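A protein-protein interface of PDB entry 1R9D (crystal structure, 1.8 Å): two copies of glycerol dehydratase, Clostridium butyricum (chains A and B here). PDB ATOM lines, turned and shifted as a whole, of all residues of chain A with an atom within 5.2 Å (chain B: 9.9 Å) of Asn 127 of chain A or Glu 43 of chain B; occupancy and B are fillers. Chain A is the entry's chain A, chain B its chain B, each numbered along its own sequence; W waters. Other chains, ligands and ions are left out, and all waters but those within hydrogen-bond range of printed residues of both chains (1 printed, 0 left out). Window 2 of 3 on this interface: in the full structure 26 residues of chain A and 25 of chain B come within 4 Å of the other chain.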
ATOM      1  N   LYS A  92      -3.440  19.656   1.469  1.00  0.00           N
ATOM      2  CA  LYS A  92      -3.593  21.069   1.783  1.00  0.00           C
ATOM      3  C   LYS A  92      -5.054  21.435   2.043  1.00  0.00           C
ATOM      4  O   LYS A  92      -5.338  22.366   2.796  1.00  0.00           O
ATOM      5  CB  LYS A  92      -3.017  21.930   0.656  1.00  0.00           C
ATOM      6  CG  LYS A  92      -1.490  21.861   0.563  1.00  0.00           C
ATOM      7  CD  LYS A  92      -0.945  22.770  -0.527  1.00  0.00           C
ATOM      8  CE  LYS A  92       0.558  22.567  -0.724  1.00  0.00           C
ATOM      9  NZ  LYS A  92       1.336  22.823   0.526  1.00  0.00           N
ATOM     10  N   VAL A 122       3.007  16.351   8.845  1.00  0.00           N
ATOM     11  CA  VAL A 122       2.573  15.674   7.628  1.00  0.00           C
ATOM     12  C   VAL A 122       2.431  16.697   6.502  1.00  0.00           C
ATOM     13  O   VAL A 122       2.968  16.507   5.413  1.00  0.00           O
ATOM     14  CB  VAL A 122       1.222  14.952   7.847  1.00  0.00           C
ATOM     15  CG1 VAL A 122       0.764  14.294   6.551  1.00  0.00           C
ATOM     16  CG2 VAL A 122       1.368  13.905   8.940  1.00  0.00           C
ATOM     17  N   PHE A 123       1.715  17.785   6.777  1.00  0.00           N
ATOM     18  CA  PHE A 123       1.518  18.845   5.793  1.00  0.00           C
ATOM     19  C   PHE A 123       2.865  19.405   5.346  1.00  0.00           C
ATOM     20  O   PHE A 123       3.061  19.714   4.171  1.00  0.00           O
ATOM     21  CB  PHE A 123       0.681  19.985   6.387  1.00  0.00           C
ATOM     22  CG  PHE A 123      -0.699  19.571   6.822  1.00  0.00           C
ATOM     23  CD1 PHE A 123      -1.238  20.057   8.010  1.00  0.00           C
ATOM     24  CD2 PHE A 123      -1.466  18.709   6.044  1.00  0.00           C
ATOM     25  CE1 PHE A 123      -2.519  19.691   8.420  1.00  0.00           C
ATOM     26  CE2 PHE A 123      -2.751  18.336   6.443  1.00  0.00           C
ATOM     27  CZ  PHE A 123      -3.278  18.828   7.633  1.00  0.00           C
ATOM     28  N   GLU A 124       3.792  19.535   6.291  1.00  0.00           N
ATOM     29  CA  GLU A 124       5.113  20.068   5.982  1.00  0.00           C
ATOM     30  C   GLU A 124       5.920  19.153   5.065  1.00  0.00           C
ATOM     31  O   GLU A 124       6.505  19.611   4.086  1.00  0.00           O
ATOM     32  CB  GLU A 124       5.898  20.318   7.272  1.00  0.00           C
ATOM     33  CG  GLU A 124       7.228  21.018   7.058  1.00  0.00           C
ATOM     34  CD  GLU A 124       8.002  21.201   8.353  1.00  0.00           C
ATOM     35  OE1 GLU A 124       7.428  21.753   9.319  1.00  0.00           O
ATOM     36  OE2 GLU A 124       9.185  20.796   8.403  1.00  0.00           O
ATOM     37  N   TYR A 125       5.954  17.862   5.370  1.00  0.00           N
ATOM     38  CA  TYR A 125       6.723  16.941   4.542  1.00  0.00           C
ATOM     39  C   TYR A 125       6.197  16.793   3.119  1.00  0.00           C
ATOM     40  O   TYR A 125       6.960  16.893   2.158  1.00  0.00           O
ATOM     41  CB  TYR A 125       6.779  15.541   5.155  1.00  0.00           C
ATOM     42  CG  TYR A 125       7.482  14.557   4.235  1.00  0.00           C
ATOM     43  CD1 TYR A 125       8.870  14.577   4.094  1.00  0.00           C
ATOM     44  CD2 TYR A 125       6.754  13.671   3.440  1.00  0.00           C
ATOM     45  CE1 TYR A 125       9.516  13.743   3.185  1.00  0.00           C
ATOM     46  CE2 TYR A 125       7.391  12.831   2.522  1.00  0.00           C
ATOM     47  CZ  TYR A 125       8.772  12.875   2.401  1.00  0.00           C
ATOM     48  OH  TYR A 125       9.408  12.066   1.487  1.00  0.00           O
ATOM     49  N   TRP A 126       4.897  16.549   2.986  1.00  0.00           N
ATOM     50  CA  TRP A 126       4.306  16.326   1.669  1.00  0.00           C
ATOM     51  C   TRP A 126       4.134  17.521   0.751  1.00  0.00           C
ATOM     52  O   TRP A 126       3.626  17.383  -0.361  1.00  0.00           O
ATOM     53  CB  TRP A 126       2.970  15.604   1.817  1.00  0.00           C
ATOM     54  CG  TRP A 126       3.118  14.229   2.370  1.00  0.00           C
ATOM     55  CD1 TRP A 126       3.046  13.858   3.682  1.00  0.00           C
ATOM     56  CD2 TRP A 126       3.402  13.035   1.630  1.00  0.00           C
ATOM     57  NE1 TRP A 126       3.265  12.509   3.804  1.00  0.00           N
ATOM     58  CE2 TRP A 126       3.487  11.979   2.560  1.00  0.00           C
ATOM     59  CE3 TRP A 126       3.594  12.758   0.267  1.00  0.00           C
ATOM     60  CZ2 TRP A 126       3.757  10.657   2.176  1.00  0.00           C
ATOM     61  CZ3 TRP A 126       3.862  11.443  -0.117  1.00  0.00           C
ATOM     62  CH2 TRP A 126       3.940  10.411   0.835  1.00  0.00           C
ATOM     63  N   ASN A 127       4.564  18.694   1.194  1.00  0.00           N
ATOM     64  CA  ASN A 127       4.439  19.877   0.361  1.00  0.00           C
ATOM     65  C   ASN A 127       5.176  19.700  -0.969  1.00  0.00           C
ATOM     66  O   ASN A 127       6.399  19.526  -0.999  1.00  0.00           O
ATOM     67  CB  ASN A 127       4.980  21.103   1.097  1.00  0.00           C
ATOM     68  CG  ASN A 127       4.883  22.361   0.268  1.00  0.00           C
ATOM     69  OD1 ASN A 127       3.830  22.673  -0.284  1.00  0.00           O
ATOM     70  ND2 ASN A 127       5.986  23.097   0.175  1.00  0.00           N
ATOM     71  N   GLY A 128       4.418  19.742  -2.062  1.00  0.00           N
ATOM     72  CA  GLY A 128       4.986  19.597  -3.390  1.00  0.00           C
ATOM     73  C   GLY A 128       5.288  18.169  -3.814  1.00  0.00           C
ATOM     74  O   GLY A 128       5.755  17.943  -4.927  1.00  0.00           O
ATOM     75  N   LYS A 129       4.993  17.199  -2.956  1.00  0.00           N
ATOM     76  CA  LYS A 129       5.301  15.805  -3.262  1.00  0.00           C
ATOM     77  C   LYS A 129       4.109  14.891  -3.525  1.00  0.00           C
ATOM     78  O   LYS A 129       4.271  13.673  -3.622  1.00  0.00           O
ATOM     79  CB  LYS A 129       6.137  15.224  -2.119  1.00  0.00           C
ATOM     80  CG  LYS A 129       7.365  16.062  -1.800  1.00  0.00           C
ATOM     81  CD  LYS A 129       8.097  15.539  -0.580  1.00  0.00           C
ATOM     82  CE  LYS A 129       9.241  16.470  -0.198  1.00  0.00           C
ATOM     83  NZ  LYS A 129       9.836  16.089   1.114  1.00  0.00           N
ATOM     84  N   GLU A 133      -0.230  17.714  -6.926  1.00  0.00           N
ATOM     85  CA  GLU A 133       0.661  18.800  -7.314  1.00  0.00           C
ATOM     86  C   GLU A 133       1.386  18.519  -8.631  1.00  0.00           C
ATOM     87  O   GLU A 133       1.569  19.421  -9.448  1.00  0.00           O
ATOM     88  CB  GLU A 133       1.634  19.090  -6.162  1.00  0.00           C
ATOM     89  CG  GLU A 133       0.864  19.566  -4.923  1.00  0.00           C
ATOM     90  CD  GLU A 133       1.674  19.562  -3.641  1.00  0.00           C
ATOM     91  OE1 GLU A 133       2.103  20.654  -3.204  1.00  0.00           O
ATOM     92  OE2 GLU A 133       1.874  18.466  -3.070  1.00  0.00           O
ATOM     93  N   ARG A 516       4.052   8.931  -9.317  1.00  0.00           N
ATOM     94  CA  ARG A 516       4.217   9.016  -7.869  1.00  0.00           C
ATOM     95  C   ARG A 516       3.471   8.017  -6.996  1.00  0.00           C
ATOM     96  O   ARG A 516       3.848   7.819  -5.837  1.00  0.00           O
ATOM     97  CB  ARG A 516       3.899  10.439  -7.408  1.00  0.00           C
ATOM     98  CG  ARG A 516       4.922  11.452  -7.896  1.00  0.00           C
ATOM     99  CD  ARG A 516       4.673  12.855  -7.361  1.00  0.00           C
ATOM    100  NE  ARG A 516       5.758  13.750  -7.759  1.00  0.00           N
ATOM    101  CZ  ARG A 516       5.860  15.025  -7.397  1.00  0.00           C
ATOM    102  NH1 ARG A 516       4.935  15.577  -6.621  1.00  0.00           N
ATOM    103  NH2 ARG A 516       6.897  15.746  -7.806  1.00  0.00           N
ATOM    104  N   ILE B  35      21.466  25.697  -6.782  1.00  0.00           N
ATOM    105  CA  ILE B  35      20.650  24.598  -7.281  1.00  0.00           C
ATOM    106  C   ILE B  35      19.781  24.060  -6.141  1.00  0.00           C
ATOM    107  O   ILE B  35      18.657  23.608  -6.362  1.00  0.00           O
ATOM    108  CB  ILE B  35      21.529  23.468  -7.897  1.00  0.00           C
ATOM    109  CG1 ILE B  35      20.638  22.479  -8.648  1.00  0.00           C
ATOM    110  CG2 ILE B  35      22.327  22.754  -6.815  1.00  0.00           C
ATOM    111  CD1 ILE B  35      21.401  21.555  -9.583  1.00  0.00           C
ATOM    112  N   THR B  36      20.294  24.139  -4.913  1.00  0.00           N
ATOM    113  CA  THR B  36      19.554  23.677  -3.747  1.00  0.00           C
ATOM    114  C   THR B  36      18.344  24.589  -3.540  1.00  0.00           C
ATOM    115  O   THR B  36      17.237  24.118  -3.281  1.00  0.00           O
ATOM    116  CB  THR B  36      20.442  23.689  -2.478  1.00  0.00           C
ATOM    117  OG1 THR B  36      21.502  22.733  -2.631  1.00  0.00           O
ATOM    118  CG2 THR B  36      19.625  23.328  -1.246  1.00  0.00           C
ATOM    119  N   GLU B  37      18.564  25.895  -3.670  1.00  0.00           N
ATOM    120  CA  GLU B  37      17.490  26.877  -3.522  1.00  0.00           C
ATOM    121  C   GLU B  37      16.361  26.559  -4.490  1.00  0.00           C
ATOM    122  O   GLU B  37      15.191  26.504  -4.109  1.00  0.00           O
ATOM    123  CB  GLU B  37      17.986  28.281  -3.859  1.00  0.00           C
ATOM    124  CG  GLU B  37      18.817  28.966  -2.808  1.00  0.00           C
ATOM    125  CD  GLU B  37      19.334  30.306  -3.302  1.00  0.00           C
ATOM    126  OE1 GLU B  37      18.531  31.088  -3.861  1.00  0.00           O
ATOM    127  OE2 GLU B  37      20.541  30.582  -3.132  1.00  0.00           O
ATOM    128  N   SER B  38      16.729  26.376  -5.754  1.00  0.00           N
ATOM    129  CA  SER B  38      15.761  26.095  -6.806  1.00  0.00           C
ATOM    130  C   SER B  38      14.976  24.806  -6.603  1.00  0.00           C
ATOM    131  O   SER B  38      13.745  24.809  -6.687  1.00  0.00           O
ATOM    132  CB  SER B  38      16.458  26.055  -8.167  1.00  0.00           C
ATOM    133  OG  SER B  38      15.511  25.862  -9.203  1.00  0.00           O
ATOM    134  N   PHE B  39      15.671  23.702  -6.345  1.00  0.00           N
ATOM    135  CA  PHE B  39      14.970  22.438  -6.150  1.00  0.00           C
ATOM    136  C   PHE B  39      13.957  22.496  -5.010  1.00  0.00           C
ATOM    137  O   PHE B  39      12.908  21.859  -5.078  1.00  0.00           O
ATOM    138  CB  PHE B  39      15.960  21.293  -5.925  1.00  0.00           C
ATOM    139  CG  PHE B  39      16.288  20.524  -7.181  1.00  0.00           C
ATOM    140  CD1 PHE B  39      16.848  21.166  -8.280  1.00  0.00           C
ATOM    141  CD2 PHE B  39      16.010  19.161  -7.268  1.00  0.00           C
ATOM    142  CE1 PHE B  39      17.129  20.459  -9.458  1.00  0.00           C
ATOM    143  CE2 PHE B  39      16.286  18.449  -8.439  1.00  0.00           C
ATOM    144  CZ  PHE B  39      16.845  19.102  -9.532  1.00  0.00           C
ATOM    145  N   LYS B  40      14.264  23.261  -3.967  1.00  0.00           N
ATOM    146  CA  LYS B  40      13.342  23.378  -2.845  1.00  0.00           C
ATOM    147  C   LYS B  40      12.033  24.034  -3.274  1.00  0.00           C
ATOM    148  O   LYS B  40      11.000  23.848  -2.630  1.00  0.00           O
ATOM    149  CB  LYS B  40      13.973  24.196  -1.714  1.00  0.00           C
ATOM    150  CG  LYS B  40      14.999  23.438  -0.888  1.00  0.00           C
ATOM    151  CD  LYS B  40      15.584  24.327   0.205  1.00  0.00           C
ATOM    152  CE  LYS B  40      16.559  23.561   1.087  1.00  0.00           C
ATOM    153  NZ  LYS B  40      17.231  24.472   2.062  1.00  0.00           N
ATOM    154  N   GLN B  41      12.076  24.795  -4.363  1.00  0.00           N
ATOM    155  CA  GLN B  41      10.893  25.493  -4.849  1.00  0.00           C
ATOM    156  C   GLN B  41      10.180  24.822  -6.019  1.00  0.00           C
ATOM    157  O   GLN B  41       9.142  25.307  -6.467  1.00  0.00           O
ATOM    158  CB  GLN B  41      11.267  26.919  -5.261  1.00  0.00           C
ATOM    159  CG  GLN B  41      11.826  27.773  -4.140  1.00  0.00           C
ATOM    160  CD  GLN B  41      10.871  27.886  -2.972  1.00  0.00           C
ATOM    161  OE1 GLN B  41       9.694  28.204  -3.150  1.00  0.00           O
ATOM    162  NE2 GLN B  41      11.371  27.628  -1.767  1.00  0.00           N
ATOM    163  N   THR B  42      10.722  23.712  -6.513  1.00  0.00           N
ATOM    164  CA  THR B  42      10.117  23.027  -7.655  1.00  0.00           C
ATOM    165  C   THR B  42       9.784  21.566  -7.380  1.00  0.00           C
ATOM    166  O   THR B  42       9.771  20.742  -8.293  1.00  0.00           O
ATOM    167  CB  THR B  42      11.051  23.087  -8.882  1.00  0.00           C
ATOM    168  OG1 THR B  42      12.301  22.462  -8.562  1.00  0.00           O
ATOM    169  CG2 THR B  42      11.297  24.527  -9.294  1.00  0.00           C
ATOM    170  N   GLU B  43       9.504  21.253  -6.123  1.00  0.00           N
ATOM    171  CA  GLU B  43       9.183  19.892  -5.711  1.00  0.00           C
ATOM    172  C   GLU B  43       8.053  19.238  -6.521  1.00  0.00           C
ATOM    173  O   GLU B  43       8.110  18.044  -6.817  1.00  0.00           O
ATOM    174  CB  GLU B  43       8.807  19.897  -4.229  1.00  0.00           C
ATOM    175  CG  GLU B  43       9.249  18.672  -3.453  1.00  0.00           C
ATOM    176  CD  GLU B  43      10.762  18.572  -3.315  1.00  0.00           C
ATOM    177  OE1 GLU B  43      11.387  19.511  -2.773  1.00  0.00           O
ATOM    178  OE2 GLU B  43      11.323  17.549  -3.743  1.00  0.00           O
ATOM    179  N   GLY B  44       7.035  20.012  -6.884  1.00  0.00           N
ATOM    180  CA  GLY B  44       5.913  19.447  -7.624  1.00  0.00           C
ATOM    181  C   GLY B  44       6.017  19.468  -9.137  1.00  0.00           C
ATOM    182  O   GLY B  44       5.032  19.226  -9.836  1.00  0.00           O
ATOM    183  N   GLN B  45       7.218  19.725  -9.638  1.00  0.00           N
ATOM    184  CA  GLN B  45       7.493  19.819 -11.070  1.00  0.00           C
ATOM    185  C   GLN B  45       8.172  18.544 -11.595  1.00  0.00           C
ATOM    186  O   GLN B  45       8.881  17.865 -10.858  1.00  0.00           O
ATOM    187  CB  GLN B  45       8.421  21.017 -11.295  1.00  0.00           C
ATOM    188  CG  GLN B  45       8.254  21.769 -12.592  1.00  0.00           C
ATOM    189  CD  GLN B  45       6.921  22.481 -12.687  1.00  0.00           C
ATOM    190  OE1 GLN B  45       6.070  22.103 -13.479  1.00  0.00           O
ATOM    191  NE2 GLN B  45       6.733  23.512 -11.870  1.00  0.00           N
ATOM    192  N   PRO B  46       7.949  18.201 -12.878  1.00  0.00           N
ATOM    193  CA  PRO B  46       8.567  17.007 -13.469  1.00  0.00           C
ATOM    194  C   PRO B  46      10.079  17.248 -13.479  1.00  0.00           C
ATOM    195  O   PRO B  46      10.519  18.393 -13.562  1.00  0.00           O
ATOM    196  CB  PRO B  46       7.997  16.981 -14.887  1.00  0.00           C
ATOM    197  CG  PRO B  46       6.697  17.696 -14.755  1.00  0.00           C
ATOM    198  CD  PRO B  46       7.014  18.831 -13.825  1.00  0.00           C
ATOM    199  N   ALA B  47      10.872  16.185 -13.419  1.00  0.00           N
ATOM    200  CA  ALA B  47      12.327  16.329 -13.394  1.00  0.00           C
ATOM    201  C   ALA B  47      12.915  17.245 -14.465  1.00  0.00           C
ATOM    202  O   ALA B  47      13.791  18.056 -14.174  1.00  0.00           O
ATOM    203  CB  ALA B  47      12.986  14.957 -13.476  1.00  0.00           C
ATOM    204  N   LEU B  49      11.659  19.824 -15.947  1.00  0.00           N
ATOM    205  CA  LEU B  49      11.429  21.239 -15.660  1.00  0.00           C
ATOM    206  C   LEU B  49      12.246  21.689 -14.449  1.00  0.00           C
ATOM    207  O   LEU B  49      12.716  22.827 -14.404  1.00  0.00           O
ATOM    208  CB  LEU B  49       9.941  21.515 -15.426  1.00  0.00           C
ATOM    209  CG  LEU B  49       9.105  21.755 -16.685  1.00  0.00           C
ATOM    210  CD1 LEU B  49       7.628  21.807 -16.322  1.00  0.00           C
ATOM    211  CD2 LEU B  49       9.544  23.062 -17.346  1.00  0.00           C
ATOM    212  N   ARG B  50      12.419  20.808 -13.469  1.00  0.00           N
ATOM    213  CA  ARG B  50      13.217  21.167 -12.301  1.00  0.00           C
ATOM    214  C   ARG B  50      14.637  21.462 -12.772  1.00  0.00           C
ATOM    215  O   ARG B  50      15.280  22.389 -12.284  1.00  0.00           O
ATOM    216  CB  ARG B  50      13.236  20.035 -11.273  1.00  0.00           C
ATOM    217  CG  ARG B  50      11.865  19.706 -10.693  1.00  0.00           C
ATOM    218  CD  ARG B  50      11.973  18.679  -9.592  1.00  0.00           C
ATOM    219  NE  ARG B  50      12.385  19.274  -8.322  1.00  0.00           N
ATOM    220  CZ  ARG B  50      12.673  18.570  -7.233  1.00  0.00           C
ATOM    221  NH1 ARG B  50      12.604  17.244  -7.261  1.00  0.00           N
ATOM    222  NH2 ARG B  50      13.006  19.193  -6.109  1.00  0.00           N
ATOM    223  N   ARG B  51      15.114  20.678 -13.739  1.00  0.00           N
ATOM    224  CA  ARG B  51      16.457  20.867 -14.282  1.00  0.00           C
ATOM    225  C   ARG B  51      16.579  22.186 -15.050  1.00  0.00           C
ATOM    226  O   ARG B  51      17.600  22.867 -14.967  1.00  0.00           O
ATOM    227  CB  ARG B  51      16.832  19.702 -15.209  1.00  0.00           C
ATOM    228  CG  ARG B  51      17.039  18.356 -14.518  1.00  0.00           C
ATOM    229  CD  ARG B  51      18.210  18.383 -13.530  1.00  0.00           C
ATOM    230  NE  ARG B  51      19.390  19.019 -14.107  1.00  0.00           N
ATOM    231  CZ  ARG B  51      20.570  19.116 -13.499  1.00  0.00           C
ATOM    232  NH1 ARG B  51      20.745  18.610 -12.286  1.00  0.00           N
ATOM    233  NH2 ARG B  51      21.571  19.741 -14.101  1.00  0.00           N
ATOM    234  N   LEU B  53      14.595  24.909 -14.649  1.00  0.00           N
ATOM    235  CA  LEU B  53      14.411  26.010 -13.704  1.00  0.00           C
ATOM    236  C   LEU B  53      15.636  26.188 -12.811  1.00  0.00           C
ATOM    237  O   LEU B  53      15.943  27.304 -12.379  1.00  0.00           O
ATOM    238  CB  LEU B  53      13.162  25.770 -12.848  1.00  0.00           C
ATOM    239  CG  LEU B  53      11.840  25.787 -13.625  1.00  0.00           C
ATOM    240  CD1 LEU B  53      10.700  25.354 -12.727  1.00  0.00           C
ATOM    241  CD2 LEU B  53      11.590  27.182 -14.181  1.00  0.00           C
ATOM    242  N   TYR B 125      19.829  18.639   2.452  1.00  0.00           N
ATOM    243  CA  TYR B 125      18.742  18.582   1.483  1.00  0.00           C
ATOM    244  C   TYR B 125      18.828  17.424   0.502  1.00  0.00           C
ATOM    245  O   TYR B 125      17.844  16.719   0.276  1.00  0.00           O
ATOM    246  CB  TYR B 125      18.656  19.869   0.663  1.00  0.00           C
ATOM    247  CG  TYR B 125      17.603  19.765  -0.419  1.00  0.00           C
ATOM    248  CD1 TYR B 125      16.246  19.834  -0.103  1.00  0.00           C
ATOM    249  CD2 TYR B 125      17.960  19.508  -1.748  1.00  0.00           C
ATOM    250  CE1 TYR B 125      15.268  19.645  -1.076  1.00  0.00           C
ATOM    251  CE2 TYR B 125      16.987  19.315  -2.730  1.00  0.00           C
ATOM    252  CZ  TYR B 125      15.644  19.383  -2.385  1.00  0.00           C
ATOM    253  OH  TYR B 125      14.676  19.175  -3.339  1.00  0.00           O
ATOM    254  N   TRP B 126      20.005  17.234  -0.085  1.00  0.00           N
ATOM    255  CA  TRP B 126      20.175  16.188  -1.086  1.00  0.00           C
ATOM    256  C   TRP B 126      20.247  14.748  -0.607  1.00  0.00           C
ATOM    257  O   TRP B 126      20.390  13.837  -1.421  1.00  0.00           O
ATOM    258  CB  TRP B 126      21.391  16.498  -1.963  1.00  0.00           C
ATOM    259  CG  TRP B 126      21.188  17.711  -2.818  1.00  0.00           C
ATOM    260  CD1 TRP B 126      21.535  19.001  -2.517  1.00  0.00           C
ATOM    261  CD2 TRP B 126      20.529  17.759  -4.090  1.00  0.00           C
ATOM    262  NE1 TRP B 126      21.129  19.847  -3.524  1.00  0.00           N
ATOM    263  CE2 TRP B 126      20.509  19.111  -4.500  1.00  0.00           C
ATOM    264  CE3 TRP B 126      19.950  16.789  -4.923  1.00  0.00           C
ATOM    265  CZ2 TRP B 126      19.932  19.519  -5.709  1.00  0.00           C
ATOM    266  CZ3 TRP B 126      19.377  17.196  -6.124  1.00  0.00           C
ATOM    267  CH2 TRP B 126      19.372  18.549  -6.505  1.00  0.00           C
ATOM    268  N   ASN B 127      20.136  14.525   0.698  1.00  0.00           N
ATOM    269  CA  ASN B 127      20.190  13.164   1.212  1.00  0.00           C
ATOM    270  C   ASN B 127      19.111  12.288   0.578  1.00  0.00           C
ATOM    271  O   ASN B 127      17.915  12.522   0.763  1.00  0.00           O
ATOM    272  CB  ASN B 127      20.031  13.151   2.736  1.00  0.00           C
ATOM    273  CG  ASN B 127      20.025  11.745   3.303  1.00  0.00           C
ATOM    274  OD1 ASN B 127      20.943  10.963   3.061  1.00  0.00           O
ATOM    275  ND2 ASN B 127      18.984  11.414   4.061  1.00  0.00           N
ATOM    276  N   GLY B 128      19.548  11.280  -0.172  1.00  0.00           N
ATOM    277  CA  GLY B 128      18.630  10.363  -0.823  1.00  0.00           C
ATOM    278  C   GLY B 128      18.005  10.857  -2.114  1.00  0.00           C
ATOM    279  O   GLY B 128      17.205  10.149  -2.715  1.00  0.00           O
ATOM    280  N   LYS B 129      18.381  12.051  -2.563  1.00  0.00           N
ATOM    281  CA  LYS B 129      17.789  12.617  -3.774  1.00  0.00           C
ATOM    282  C   LYS B 129      18.726  12.740  -4.973  1.00  0.00           C
ATOM    283  O   LYS B 129      18.381  13.382  -5.966  1.00  0.00           O
ATOM    284  CB  LYS B 129      17.213  13.996  -3.449  1.00  0.00           C
ATOM    285  CG  LYS B 129      16.237  13.973  -2.286  1.00  0.00           C
ATOM    286  CD  LYS B 129      15.910  15.371  -1.805  1.00  0.00           C
ATOM    287  CE  LYS B 129      15.069  15.316  -0.537  1.00  0.00           C
ATOM    288  NZ  LYS B 129      14.936  16.656   0.093  1.00  0.00           N
ATOM    289  N   ARG B 516      16.352  11.278 -12.801  1.00  0.00           N
ATOM    290  CA  ARG B 516      16.594  12.444 -11.960  1.00  0.00           C
ATOM    291  C   ARG B 516      17.404  13.591 -12.545  1.00  0.00           C
ATOM    292  O   ARG B 516      17.333  14.712 -12.037  1.00  0.00           O
ATOM    293  CB  ARG B 516      17.221  11.995 -10.637  1.00  0.00           C
ATOM    294  CG  ARG B 516      16.279  11.146  -9.802  1.00  0.00           C
ATOM    295  CD  ARG B 516      16.865  10.745  -8.457  1.00  0.00           C
ATOM    296  NE  ARG B 516      15.852  10.091  -7.630  1.00  0.00           N
ATOM    297  CZ  ARG B 516      16.024   9.749  -6.356  1.00  0.00           C
ATOM    298  NH1 ARG B 516      17.180   9.996  -5.752  1.00  0.00           N
ATOM    299  NH2 ARG B 516      15.034   9.175  -5.683  1.00  0.00           N
HETATM  300  O   HOH W   1       9.341  15.336  -9.973  1.00  0.00           O
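Printed residues of chain B that touch a printed residue of chain A: Glu 43 and Gly 44.
Of the 11 printed residues of chain A, 5 touch a printed residue of chain B.
Among the printed residues, 7 pairs touch across the chains.
Among the printed residues, no Asp or Glu carboxylate lies within 4 Å of a Lys or Arg side-chain nitrogen of the other chain.
Asn 127 of chain A touches one residue of chain B.
Of chain B, only Glu 43 (3.0 Å) and Gly 44 (3.1 Å) come within 4 Å of Gly 128 of chain A.
Of the printed residues of chain B, Lys 129 of chain A touches Glu 43 (3.6 Å).
Printed residues of chain B within 4 Å of Glu 133 of chain A: Gly 44.
Of the printed residues of chain B, Arg 516 of chain A touches Glu 43 and Gly 44.
Thr 42 of chain B touches none of the printed residues of chain A.
Glu 43 of chain B touches just these residues of chain A: Asn 127, Gly 128, Lys 129 and Arg 516.
Printed residues of chain A within 4 Å of Gly 44 of chain B: Gly 128, Glu 133 and Arg 516.
Gly 128 of chain B touches none of the printed residues of chain A.
The nearest printed residue of chain A that does not touch Glu 43 of chain B is Tyr 125 of chain A (6.3 Å).
O of Gly 128 of chain A sits close to N of Gly 44 of chain B (3.1 Å).
The backbone carbonyl oxygen of Glu 43 of chain B lies within hydrogen-bond range of the guanidinium group of Arg 516 of chain A (2.8 Å).
The backbone carbonyl oxygen (O) of Gly 128 of chain A lies close to the backbone carbonyl oxygen (O) of Glu 43 of chain B.
O of Glu 133 of chain A lies close to O of Gly 44 of chain B, 3.5 Å away.
The side-chain amino group (NZ) of Lys 92 of chain A is in hydrogen-bond range of the side-chain amide oxygen (OD1) of Asn 127 of chain A, 2.6 Å away.
The backbone carbonyl oxygen (O) of Tyr 125 of chain A lies close to the side-chain amino group (NZ) of Lys 129 of chain A (3.2 Å).
The guanidinium group (NH1) of Arg 516 of chain A is in hydrogen-bond range of the backbone carbonyl oxygen (O) of Gly 128 of chain A (3.0 Å).
The side-chain carboxylate (OE2) of Glu 133 of chain A lies within hydrogen-bond range of the backbone NH (N) of Lys 129 of chain A, at 3.4 Å.
The guanidinium group (NH2) of Arg 50 of chain B lies within salt-bridge range of the side-chain carboxylate (OE2) of Glu 43 of chain B.
The side-chain carboxylate (OE1) of Glu 43 of chain B is in hydrogen-bond range of the side-chain hydroxyl (OH) of Tyr 125 of chain B, at 3.4 Å.
6 positions are printed for both chains.
Of the 7 pairs that touch across the chains among the printed residues, none has its exchanged pair printed and touching as well.
Among the printed residues, merely in contact across the chains: Lys 129 of chain A with Glu 43 of chain B (3.6 Å), Arg 516 of chain A with Gly 44 of chain B (3.8 Å) and Asn 127 of chain A with Glu 43 of chain B (3.9 Å).
Water W1 bridges O of Gln 45 of chain B (2.7 Å) and NH2 of Arg 516 of chain A (3.3 Å).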
